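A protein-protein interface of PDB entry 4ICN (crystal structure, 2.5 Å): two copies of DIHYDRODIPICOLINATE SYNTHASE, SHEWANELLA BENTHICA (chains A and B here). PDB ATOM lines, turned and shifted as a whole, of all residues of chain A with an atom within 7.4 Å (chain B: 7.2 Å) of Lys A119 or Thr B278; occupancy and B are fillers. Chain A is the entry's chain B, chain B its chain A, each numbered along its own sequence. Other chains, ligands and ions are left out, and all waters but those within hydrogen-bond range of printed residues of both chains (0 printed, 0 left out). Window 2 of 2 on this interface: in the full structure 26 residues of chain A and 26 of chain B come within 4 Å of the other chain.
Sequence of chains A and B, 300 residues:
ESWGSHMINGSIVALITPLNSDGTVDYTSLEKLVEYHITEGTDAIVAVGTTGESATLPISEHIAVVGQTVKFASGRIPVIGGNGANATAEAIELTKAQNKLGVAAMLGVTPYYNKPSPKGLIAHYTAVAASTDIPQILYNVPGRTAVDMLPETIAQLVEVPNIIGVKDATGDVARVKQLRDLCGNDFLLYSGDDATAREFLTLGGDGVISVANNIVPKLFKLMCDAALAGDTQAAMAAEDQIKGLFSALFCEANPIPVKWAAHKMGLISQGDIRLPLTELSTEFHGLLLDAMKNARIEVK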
ATOM      1  N   PRO A 116       4.765  20.037   1.352  1.00  0.00           N
ATOM      2  CA  PRO A 116       4.615  21.467   1.207  1.00  0.00           C
ATOM      3  C   PRO A 116       5.082  22.199   2.467  1.00  0.00           C
ATOM      4  O   PRO A 116       5.177  21.610   3.536  1.00  0.00           O
ATOM      5  CB  PRO A 116       3.101  21.630   1.044  1.00  0.00           C
ATOM      6  CG  PRO A 116       2.538  20.509   1.798  1.00  0.00           C
ATOM      7  CD  PRO A 116       3.487  19.367   1.670  1.00  0.00           C
ATOM      8  N   SER A 117       5.362  23.476   2.328  1.00  0.00           N
ATOM      9  CA  SER A 117       5.659  24.327   3.456  1.00  0.00           C
ATOM     10  C   SER A 117       4.401  24.765   4.249  1.00  0.00           C
ATOM     11  O   SER A 117       3.272  24.643   3.771  1.00  0.00           O
ATOM     12  CB  SER A 117       6.384  25.570   2.938  1.00  0.00           C
ATOM     13  OG  SER A 117       7.684  25.228   2.499  1.00  0.00           O
ATOM     14  N   PRO A 118       4.603  25.275   5.476  1.00  0.00           N
ATOM     15  CA  PRO A 118       3.494  25.813   6.265  1.00  0.00           C
ATOM     16  C   PRO A 118       2.583  26.757   5.450  1.00  0.00           C
ATOM     17  O   PRO A 118       1.357  26.603   5.444  1.00  0.00           O
ATOM     18  CB  PRO A 118       4.223  26.553   7.399  1.00  0.00           C
ATOM     19  CG  PRO A 118       5.462  25.723   7.621  1.00  0.00           C
ATOM     20  CD  PRO A 118       5.846  25.157   6.281  1.00  0.00           C
ATOM     21  N   LYS A 119       3.177  27.700   4.735  1.00  0.00           N
ATOM     22  CA  LYS A 119       2.414  28.637   3.890  1.00  0.00           C
ATOM     23  C   LYS A 119       1.503  27.918   2.896  1.00  0.00           C
ATOM     24  O   LYS A 119       0.414  28.400   2.552  1.00  0.00           O
ATOM     25  CB  LYS A 119       3.405  29.473   3.103  1.00  0.00           C
ATOM     26  CG  LYS A 119       2.911  30.816   2.670  1.00  0.00           C
ATOM     27  CD  LYS A 119       4.114  31.718   2.319  1.00  0.00           C
ATOM     28  CE  LYS A 119       5.130  31.008   1.386  1.00  0.00           C
ATOM     29  NZ  LYS A 119       4.843  31.286  -0.072  1.00  0.00           N
ATOM     30  N   GLY A 120       1.974  26.771   2.419  1.00  0.00           N
ATOM     31  CA  GLY A 120       1.266  25.981   1.447  1.00  0.00           C
ATOM     32  C   GLY A 120       0.137  25.213   2.076  1.00  0.00           C
ATOM     33  O   GLY A 120      -0.958  25.122   1.491  1.00  0.00           O
ATOM     34  N   LEU A 121       0.377  24.650   3.255  1.00  0.00           N
ATOM     35  CA  LEU A 121      -0.708  23.975   3.982  1.00  0.00           C
ATOM     36  C   LEU A 121      -1.872  24.930   4.238  1.00  0.00           C
ATOM     37  O   LEU A 121      -3.045  24.568   4.028  1.00  0.00           O
ATOM     38  CB  LEU A 121      -0.231  23.412   5.309  1.00  0.00           C
ATOM     39  CG  LEU A 121       0.842  22.343   5.232  1.00  0.00           C
ATOM     40  CD1 LEU A 121       1.307  21.994   6.631  1.00  0.00           C
ATOM     41  CD2 LEU A 121       0.290  21.142   4.552  1.00  0.00           C
ATOM     42  N   ILE A 122      -1.536  26.147   4.668  1.00  0.00           N
ATOM     43  CA  ILE A 122      -2.529  27.195   4.926  1.00  0.00           C
ATOM     44  C   ILE A 122      -3.345  27.495   3.667  1.00  0.00           C
ATOM     45  O   ILE A 122      -4.569  27.418   3.692  1.00  0.00           O
ATOM     46  CB  ILE A 122      -1.863  28.485   5.511  1.00  0.00           C
ATOM     47  CG1 ILE A 122      -1.421  28.219   6.959  1.00  0.00           C
ATOM     48  CG2 ILE A 122      -2.819  29.715   5.412  1.00  0.00           C
ATOM     49  CD1 ILE A 122      -0.392  29.209   7.482  1.00  0.00           C
ATOM     50  N   ALA A 123      -2.654  27.798   2.570  1.00  0.00           N
ATOM     51  CA  ALA A 123      -3.279  28.093   1.289  1.00  0.00           C
ATOM     52  C   ALA A 123      -4.083  26.887   0.819  1.00  0.00           C
ATOM     53  O   ALA A 123      -5.199  27.025   0.289  1.00  0.00           O
ATOM     54  CB  ALA A 123      -2.215  28.444   0.299  1.00  0.00           C
ATOM     55  N   HIS A 124      -3.533  25.698   1.045  1.00  0.00           N
ATOM     56  CA  HIS A 124      -4.220  24.450   0.708  1.00  0.00           C
ATOM     57  C   HIS A 124      -5.572  24.364   1.416  1.00  0.00           C
ATOM     58  O   HIS A 124      -6.609  24.337   0.807  1.00  0.00           O
ATOM     59  CB  HIS A 124      -3.319  23.218   1.054  1.00  0.00           C
ATOM     60  CG  HIS A 124      -3.991  21.898   0.855  1.00  0.00           C
ATOM     61  ND1 HIS A 124      -4.138  21.318  -0.389  1.00  0.00           N
ATOM     62  CD2 HIS A 124      -4.571  21.053   1.738  1.00  0.00           C
ATOM     63  CE1 HIS A 124      -4.776  20.165  -0.256  1.00  0.00           C
ATOM     64  NE2 HIS A 124      -5.055  19.985   1.023  1.00  0.00           N
ATOM     65  N   TYR A 125      -5.549  24.326   2.726  1.00  0.00           N
ATOM     66  CA  TYR A 125      -6.775  24.169   3.483  1.00  0.00           C
ATOM     67  C   TYR A 125      -7.759  25.364   3.313  1.00  0.00           C
ATOM     68  O   TYR A 125      -9.004  25.178   3.267  1.00  0.00           O
ATOM     69  CB  TYR A 125      -6.405  23.968   4.931  1.00  0.00           C
ATOM     70  CG  TYR A 125      -6.009  22.561   5.316  1.00  0.00           C
ATOM     71  CD1 TYR A 125      -6.895  21.493   5.168  1.00  0.00           C
ATOM     72  CD2 TYR A 125      -4.769  22.308   5.880  1.00  0.00           C
ATOM     73  CE1 TYR A 125      -6.540  20.205   5.563  1.00  0.00           C
ATOM     74  CE2 TYR A 125      -4.391  21.019   6.271  1.00  0.00           C
ATOM     75  CZ  TYR A 125      -5.282  19.976   6.119  1.00  0.00           C
ATOM     76  OH  TYR A 125      -4.935  18.707   6.556  1.00  0.00           O
ATOM     77  N   THR A 126      -7.209  26.576   3.186  1.00  0.00           N
ATOM     78  CA  THR A 126      -8.038  27.744   2.945  1.00  0.00           C
ATOM     79  C   THR A 126      -8.848  27.562   1.656  1.00  0.00           C
ATOM     80  O   THR A 126     -10.079  27.803   1.633  1.00  0.00           O
ATOM     81  CB  THR A 126      -7.184  29.058   2.922  1.00  0.00           C
ATOM     82  OG1 THR A 126      -6.595  29.259   4.218  1.00  0.00           O
ATOM     83  CG2 THR A 126      -8.036  30.280   2.542  1.00  0.00           C
ATOM     84  N   THR A 153       0.921  26.551  12.964  1.00  0.00           N
ATOM     85  CA  THR A 153       0.343  26.579  11.625  1.00  0.00           C
ATOM     86  C   THR A 153      -1.155  26.385  11.699  1.00  0.00           C
ATOM     87  O   THR A 153      -1.907  27.104  11.063  1.00  0.00           O
ATOM     88  CB  THR A 153       1.033  25.577  10.673  1.00  0.00           C
ATOM     89  OG1 THR A 153       2.410  25.936  10.568  1.00  0.00           O
ATOM     90  CG2 THR A 153       0.444  25.667   9.303  1.00  0.00           C
ATOM     91  N   GLN A 156      -3.342  29.531  12.443  1.00  0.00           N
ATOM     92  CA  GLN A 156      -3.628  30.529  11.426  1.00  0.00           C
ATOM     93  C   GLN A 156      -4.839  30.158  10.607  1.00  0.00           C
ATOM     94  O   GLN A 156      -5.253  30.926   9.733  1.00  0.00           O
ATOM     95  CB  GLN A 156      -2.443  30.721  10.504  1.00  0.00           C
ATOM     96  CG  GLN A 156      -1.236  31.360  11.158  1.00  0.00           C
ATOM     97  CD  GLN A 156      -0.263  31.888  10.119  1.00  0.00           C
ATOM     98  OE1 GLN A 156       0.913  31.498  10.085  1.00  0.00           O
ATOM     99  NE2 GLN A 156      -0.757  32.783   9.246  1.00  0.00           N
ATOM    100  N   GLU B 252      13.814  24.320   1.072  1.00  0.00           N
ATOM    101  CA  GLU B 252      12.397  23.896   1.157  1.00  0.00           C
ATOM    102  C   GLU B 252      12.325  22.585   0.356  1.00  0.00           C
ATOM    103  O   GLU B 252      13.264  22.266  -0.399  1.00  0.00           O
ATOM    104  CB  GLU B 252      11.414  24.947   0.590  1.00  0.00           C
ATOM    105  CG  GLU B 252      11.441  26.375   1.305  1.00  0.00           C
ATOM    106  CD  GLU B 252      10.270  27.313   0.916  1.00  0.00           C
ATOM    107  OE1 GLU B 252       9.090  26.925   1.041  1.00  0.00           O
ATOM    108  OE2 GLU B 252      10.517  28.464   0.485  1.00  0.00           O
ATOM    109  N   ALA B 253      11.245  21.816   0.521  1.00  0.00           N
ATOM    110  CA  ALA B 253      11.060  20.618  -0.264  1.00  0.00           C
ATOM    111  C   ALA B 253      11.206  20.808  -1.789  1.00  0.00           C
ATOM    112  O   ALA B 253      10.640  21.726  -2.409  1.00  0.00           O
ATOM    113  CB  ALA B 253       9.742  19.923   0.074  1.00  0.00           C
ATOM    114  N   PRO B 255      10.367  20.175  -5.484  1.00  0.00           N
ATOM    115  CA  PRO B 255      11.198  21.045  -6.341  1.00  0.00           C
ATOM    116  C   PRO B 255      11.104  22.547  -6.089  1.00  0.00           C
ATOM    117  O   PRO B 255      11.491  23.332  -6.965  1.00  0.00           O
ATOM    118  CB  PRO B 255      10.654  20.756  -7.753  1.00  0.00           C
ATOM    119  CG  PRO B 255       9.200  20.516  -7.521  1.00  0.00           C
ATOM    120  CD  PRO B 255       9.124  19.778  -6.171  1.00  0.00           C
ATOM    121  N   ILE B 256      10.626  22.978  -4.929  1.00  0.00           N
ATOM    122  CA  ILE B 256      10.475  24.429  -4.716  1.00  0.00           C
ATOM    123  C   ILE B 256      11.748  25.237  -5.009  1.00  0.00           C
ATOM    124  O   ILE B 256      11.688  26.219  -5.736  1.00  0.00           O
ATOM    125  CB  ILE B 256       9.940  24.772  -3.318  1.00  0.00           C
ATOM    126  CG1 ILE B 256       8.513  24.224  -3.141  1.00  0.00           C
ATOM    127  CG2 ILE B 256      10.003  26.290  -3.073  1.00  0.00           C
ATOM    128  CD1 ILE B 256       8.160  23.998  -1.694  1.00  0.00           C
ATOM    129  N   PRO B 257      12.911  24.816  -4.463  1.00  0.00           N
ATOM    130  CA  PRO B 257      14.126  25.596  -4.724  1.00  0.00           C
ATOM    131  C   PRO B 257      14.625  25.507  -6.172  1.00  0.00           C
ATOM    132  O   PRO B 257      14.894  26.529  -6.808  1.00  0.00           O
ATOM    133  CB  PRO B 257      15.138  24.985  -3.741  1.00  0.00           C
ATOM    134  CG  PRO B 257      14.316  24.441  -2.642  1.00  0.00           C
ATOM    135  CD  PRO B 257      13.114  23.882  -3.339  1.00  0.00           C
ATOM    136  N   GLY B 271       8.170  31.142 -12.757  1.00  0.00           N
ATOM    137  CA  GLY B 271       8.493  30.287 -11.633  1.00  0.00           C
ATOM    138  C   GLY B 271       7.261  29.722 -10.951  1.00  0.00           C
ATOM    139  O   GLY B 271       7.349  29.202  -9.840  1.00  0.00           O
ATOM    140  N   ILE B 273       4.161  27.543  -9.688  1.00  0.00           N
ATOM    141  CA  ILE B 273       4.134  26.189  -9.141  1.00  0.00           C
ATOM    142  C   ILE B 273       2.754  25.886  -8.530  1.00  0.00           C
ATOM    143  O   ILE B 273       2.020  26.808  -8.151  1.00  0.00           O
ATOM    144  CB  ILE B 273       5.266  26.008  -8.106  1.00  0.00           C
ATOM    145  CG1 ILE B 273       5.610  24.522  -7.931  1.00  0.00           C
ATOM    146  CG2 ILE B 273       4.939  26.714  -6.760  1.00  0.00           C
ATOM    147  CD1 ILE B 273       6.892  24.288  -7.125  1.00  0.00           C
ATOM    148  N   ARG B 274       2.397  24.607  -8.448  1.00  0.00           N
ATOM    149  CA  ARG B 274       1.020  24.250  -8.128  1.00  0.00           C
ATOM    150  C   ARG B 274       0.811  23.922  -6.681  1.00  0.00           C
ATOM    151  O   ARG B 274       1.622  23.228  -6.054  1.00  0.00           O
ATOM    152  CB  ARG B 274       0.558  23.052  -8.933  1.00  0.00           C
ATOM    153  CG  ARG B 274      -0.292  23.386 -10.080  1.00  0.00           C
ATOM    154  CD  ARG B 274      -0.576  22.140 -10.897  1.00  0.00           C
ATOM    155  NE  ARG B 274      -0.662  22.493 -12.316  1.00  0.00           N
ATOM    156  CZ  ARG B 274      -1.275  21.782 -13.251  1.00  0.00           C
ATOM    157  NH1 ARG B 274      -1.850  20.618 -12.950  1.00  0.00           N
ATOM    158  NH2 ARG B 274      -1.288  22.246 -14.499  1.00  0.00           N
ATOM    159  N   LEU B 275      -0.302  24.406  -6.152  1.00  0.00           N
ATOM    160  CA  LEU B 275      -0.664  24.133  -4.772  1.00  0.00           C
ATOM    161  C   LEU B 275      -0.814  22.622  -4.528  1.00  0.00           C
ATOM    162  O   LEU B 275      -1.364  21.938  -5.388  1.00  0.00           O
ATOM    163  CB  LEU B 275      -1.950  24.881  -4.437  1.00  0.00           C
ATOM    164  CG  LEU B 275      -1.685  26.340  -4.037  1.00  0.00           C
ATOM    165  CD1 LEU B 275      -3.017  27.040  -3.840  1.00  0.00           C
ATOM    166  CD2 LEU B 275      -0.801  26.474  -2.784  1.00  0.00           C
ATOM    167  N   PRO B 276      -0.364  22.107  -3.351  1.00  0.00           N
ATOM    168  CA  PRO B 276       0.068  22.814  -2.124  1.00  0.00           C
ATOM    169  C   PRO B 276       1.511  23.324  -2.082  1.00  0.00           C
ATOM    170  O   PRO B 276       1.956  23.824  -1.051  1.00  0.00           O
ATOM    171  CB  PRO B 276      -0.156  21.765  -1.023  1.00  0.00           C
ATOM    172  CG  PRO B 276       0.045  20.472  -1.695  1.00  0.00           C
ATOM    173  CD  PRO B 276      -0.350  20.641  -3.152  1.00  0.00           C
ATOM    174  N   LEU B 277       2.243  23.211  -3.178  1.00  0.00           N
ATOM    175  CA  LEU B 277       3.586  23.772  -3.208  1.00  0.00           C
ATOM    176  C   LEU B 277       3.519  25.290  -3.440  1.00  0.00           C
ATOM    177  O   LEU B 277       2.561  25.767  -4.031  1.00  0.00           O
ATOM    178  CB  LEU B 277       4.467  23.072  -4.257  1.00  0.00           C
ATOM    179  CG  LEU B 277       4.745  21.586  -4.047  1.00  0.00           C
ATOM    180  CD1 LEU B 277       5.842  21.117  -5.002  1.00  0.00           C
ATOM    181  CD2 LEU B 277       5.144  21.292  -2.615  1.00  0.00           C
ATOM    182  N   THR B 278       4.519  26.033  -2.960  1.00  0.00           N
ATOM    183  CA  THR B 278       4.518  27.501  -3.059  1.00  0.00           C
ATOM    184  C   THR B 278       5.882  27.979  -3.527  1.00  0.00           C
ATOM    185  O   THR B 278       6.894  27.318  -3.251  1.00  0.00           O
ATOM    186  CB  THR B 278       4.189  28.167  -1.674  1.00  0.00           C
ATOM    187  OG1 THR B 278       4.935  27.516  -0.627  1.00  0.00           O
ATOM    188  CG2 THR B 278       2.711  28.044  -1.333  1.00  0.00           C
ATOM    189  N   GLU B 279       5.945  29.111  -4.219  1.00  0.00           N
ATOM    190  CA  GLU B 279       7.256  29.638  -4.655  1.00  0.00           C
ATOM    191  C   GLU B 279       8.257  29.802  -3.499  1.00  0.00           C
ATOM    192  O   GLU B 279       7.882  29.961  -2.359  1.00  0.00           O
ATOM    193  CB  GLU B 279       7.106  30.907  -5.497  1.00  0.00           C
ATOM    194  CG  GLU B 279       6.406  30.613  -6.836  1.00  0.00           C
ATOM    195  CD  GLU B 279       6.152  31.846  -7.726  1.00  0.00           C
ATOM    196  OE1 GLU B 279       7.069  32.705  -7.852  1.00  0.00           O
ATOM    197  OE2 GLU B 279       5.043  31.936  -8.326  1.00  0.00           O
ATOM    198  N   LEU B 280       9.538  29.694  -3.783  1.00  0.00           N
ATOM    199  CA  LEU B 280      10.516  29.724  -2.717  1.00  0.00           C
ATOM    200  C   LEU B 280      10.312  30.987  -1.884  1.00  0.00           C
ATOM    201  O   LEU B 280      10.127  32.084  -2.441  1.00  0.00           O
ATOM    202  CB  LEU B 280      11.909  29.718  -3.313  1.00  0.00           C
ATOM    203  CG  LEU B 280      13.109  29.769  -2.388  1.00  0.00           C
ATOM    204  CD1 LEU B 280      13.321  28.469  -1.675  1.00  0.00           C
ATOM    205  CD2 LEU B 280      14.291  30.103  -3.211  1.00  0.00           C
ATOM    206  N   SER B 281      10.360  30.841  -0.562  1.00  0.00           N
ATOM    207  CA  SER B 281      10.146  31.997   0.318  1.00  0.00           C
ATOM    208  C   SER B 281      11.402  32.865   0.366  1.00  0.00           C
ATOM    209  O   SER B 281      12.508  32.351   0.218  1.00  0.00           O
ATOM    210  CB  SER B 281       9.643  31.591   1.713  1.00  0.00           C
ATOM    211  OG  SER B 281      10.321  30.466   2.208  1.00  0.00           O
ATOM    212  N   THR B 282      11.208  34.177   0.548  1.00  0.00           N
ATOM    213  CA  THR B 282      12.275  35.185   0.348  1.00  0.00           C
ATOM    214  C   THR B 282      13.464  35.015   1.319  1.00  0.00           C
ATOM    215  O   THR B 282      14.629  35.251   0.968  1.00  0.00           O
ATOM    216  CB  THR B 282      11.703  36.638   0.348  1.00  0.00           C
ATOM    217  OG1 THR B 282      10.869  36.824   1.493  1.00  0.00           O
ATOM    218  CG2 THR B 282      10.847  36.888  -0.907  1.00  0.00           C
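OE1 of Glu B252 sits at hydrogen-bond distance from OG of Ser A117 (2.6 Å).
N of Ser B281 is in hydrogen-bond range of OE2 of Glu B252 (2.6 Å).
Pro B276 touches Pro A116.
Pro A116 touches Leu B277 (CA to CD2, 3.9 Å).
Lys A119 touches Thr B278.
Gly A120 touches Pro B276 (CA to O, 3.4 Å).
Gly A120 touches Thr B278 (CA to CG2, 3.8 Å).
Ala A123 touches Leu B275 (CB to CD2, 3.9 Å).
Thr B278 touches just these residues of chain A: Lys A119 (3.6 Å) and Gly A120 (3.8 Å).
Of the printed residues of chain A, Glu B252 touches Ser A117.
Of the printed residues of chain B, Pro A116 touches Pro B276 and Leu B277.
Of the printed residues of chain B, Ala A123 touches Leu B275.
Of the printed residues of chain A, Leu B275 touches Ala A123.
The nearest residue of chain B that does not touch Lys A119 is Glu B279 (4.03 Å).
Hydrophobic or aromatic side chains of chain B that line the printed part of chain A: Leu B275, Pro B276 and Leu B277.
No position is printed for both chains.
Of the 7 pairs that touch across the chains among the printed residues, none has its exchanged pair printed and touching as well.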
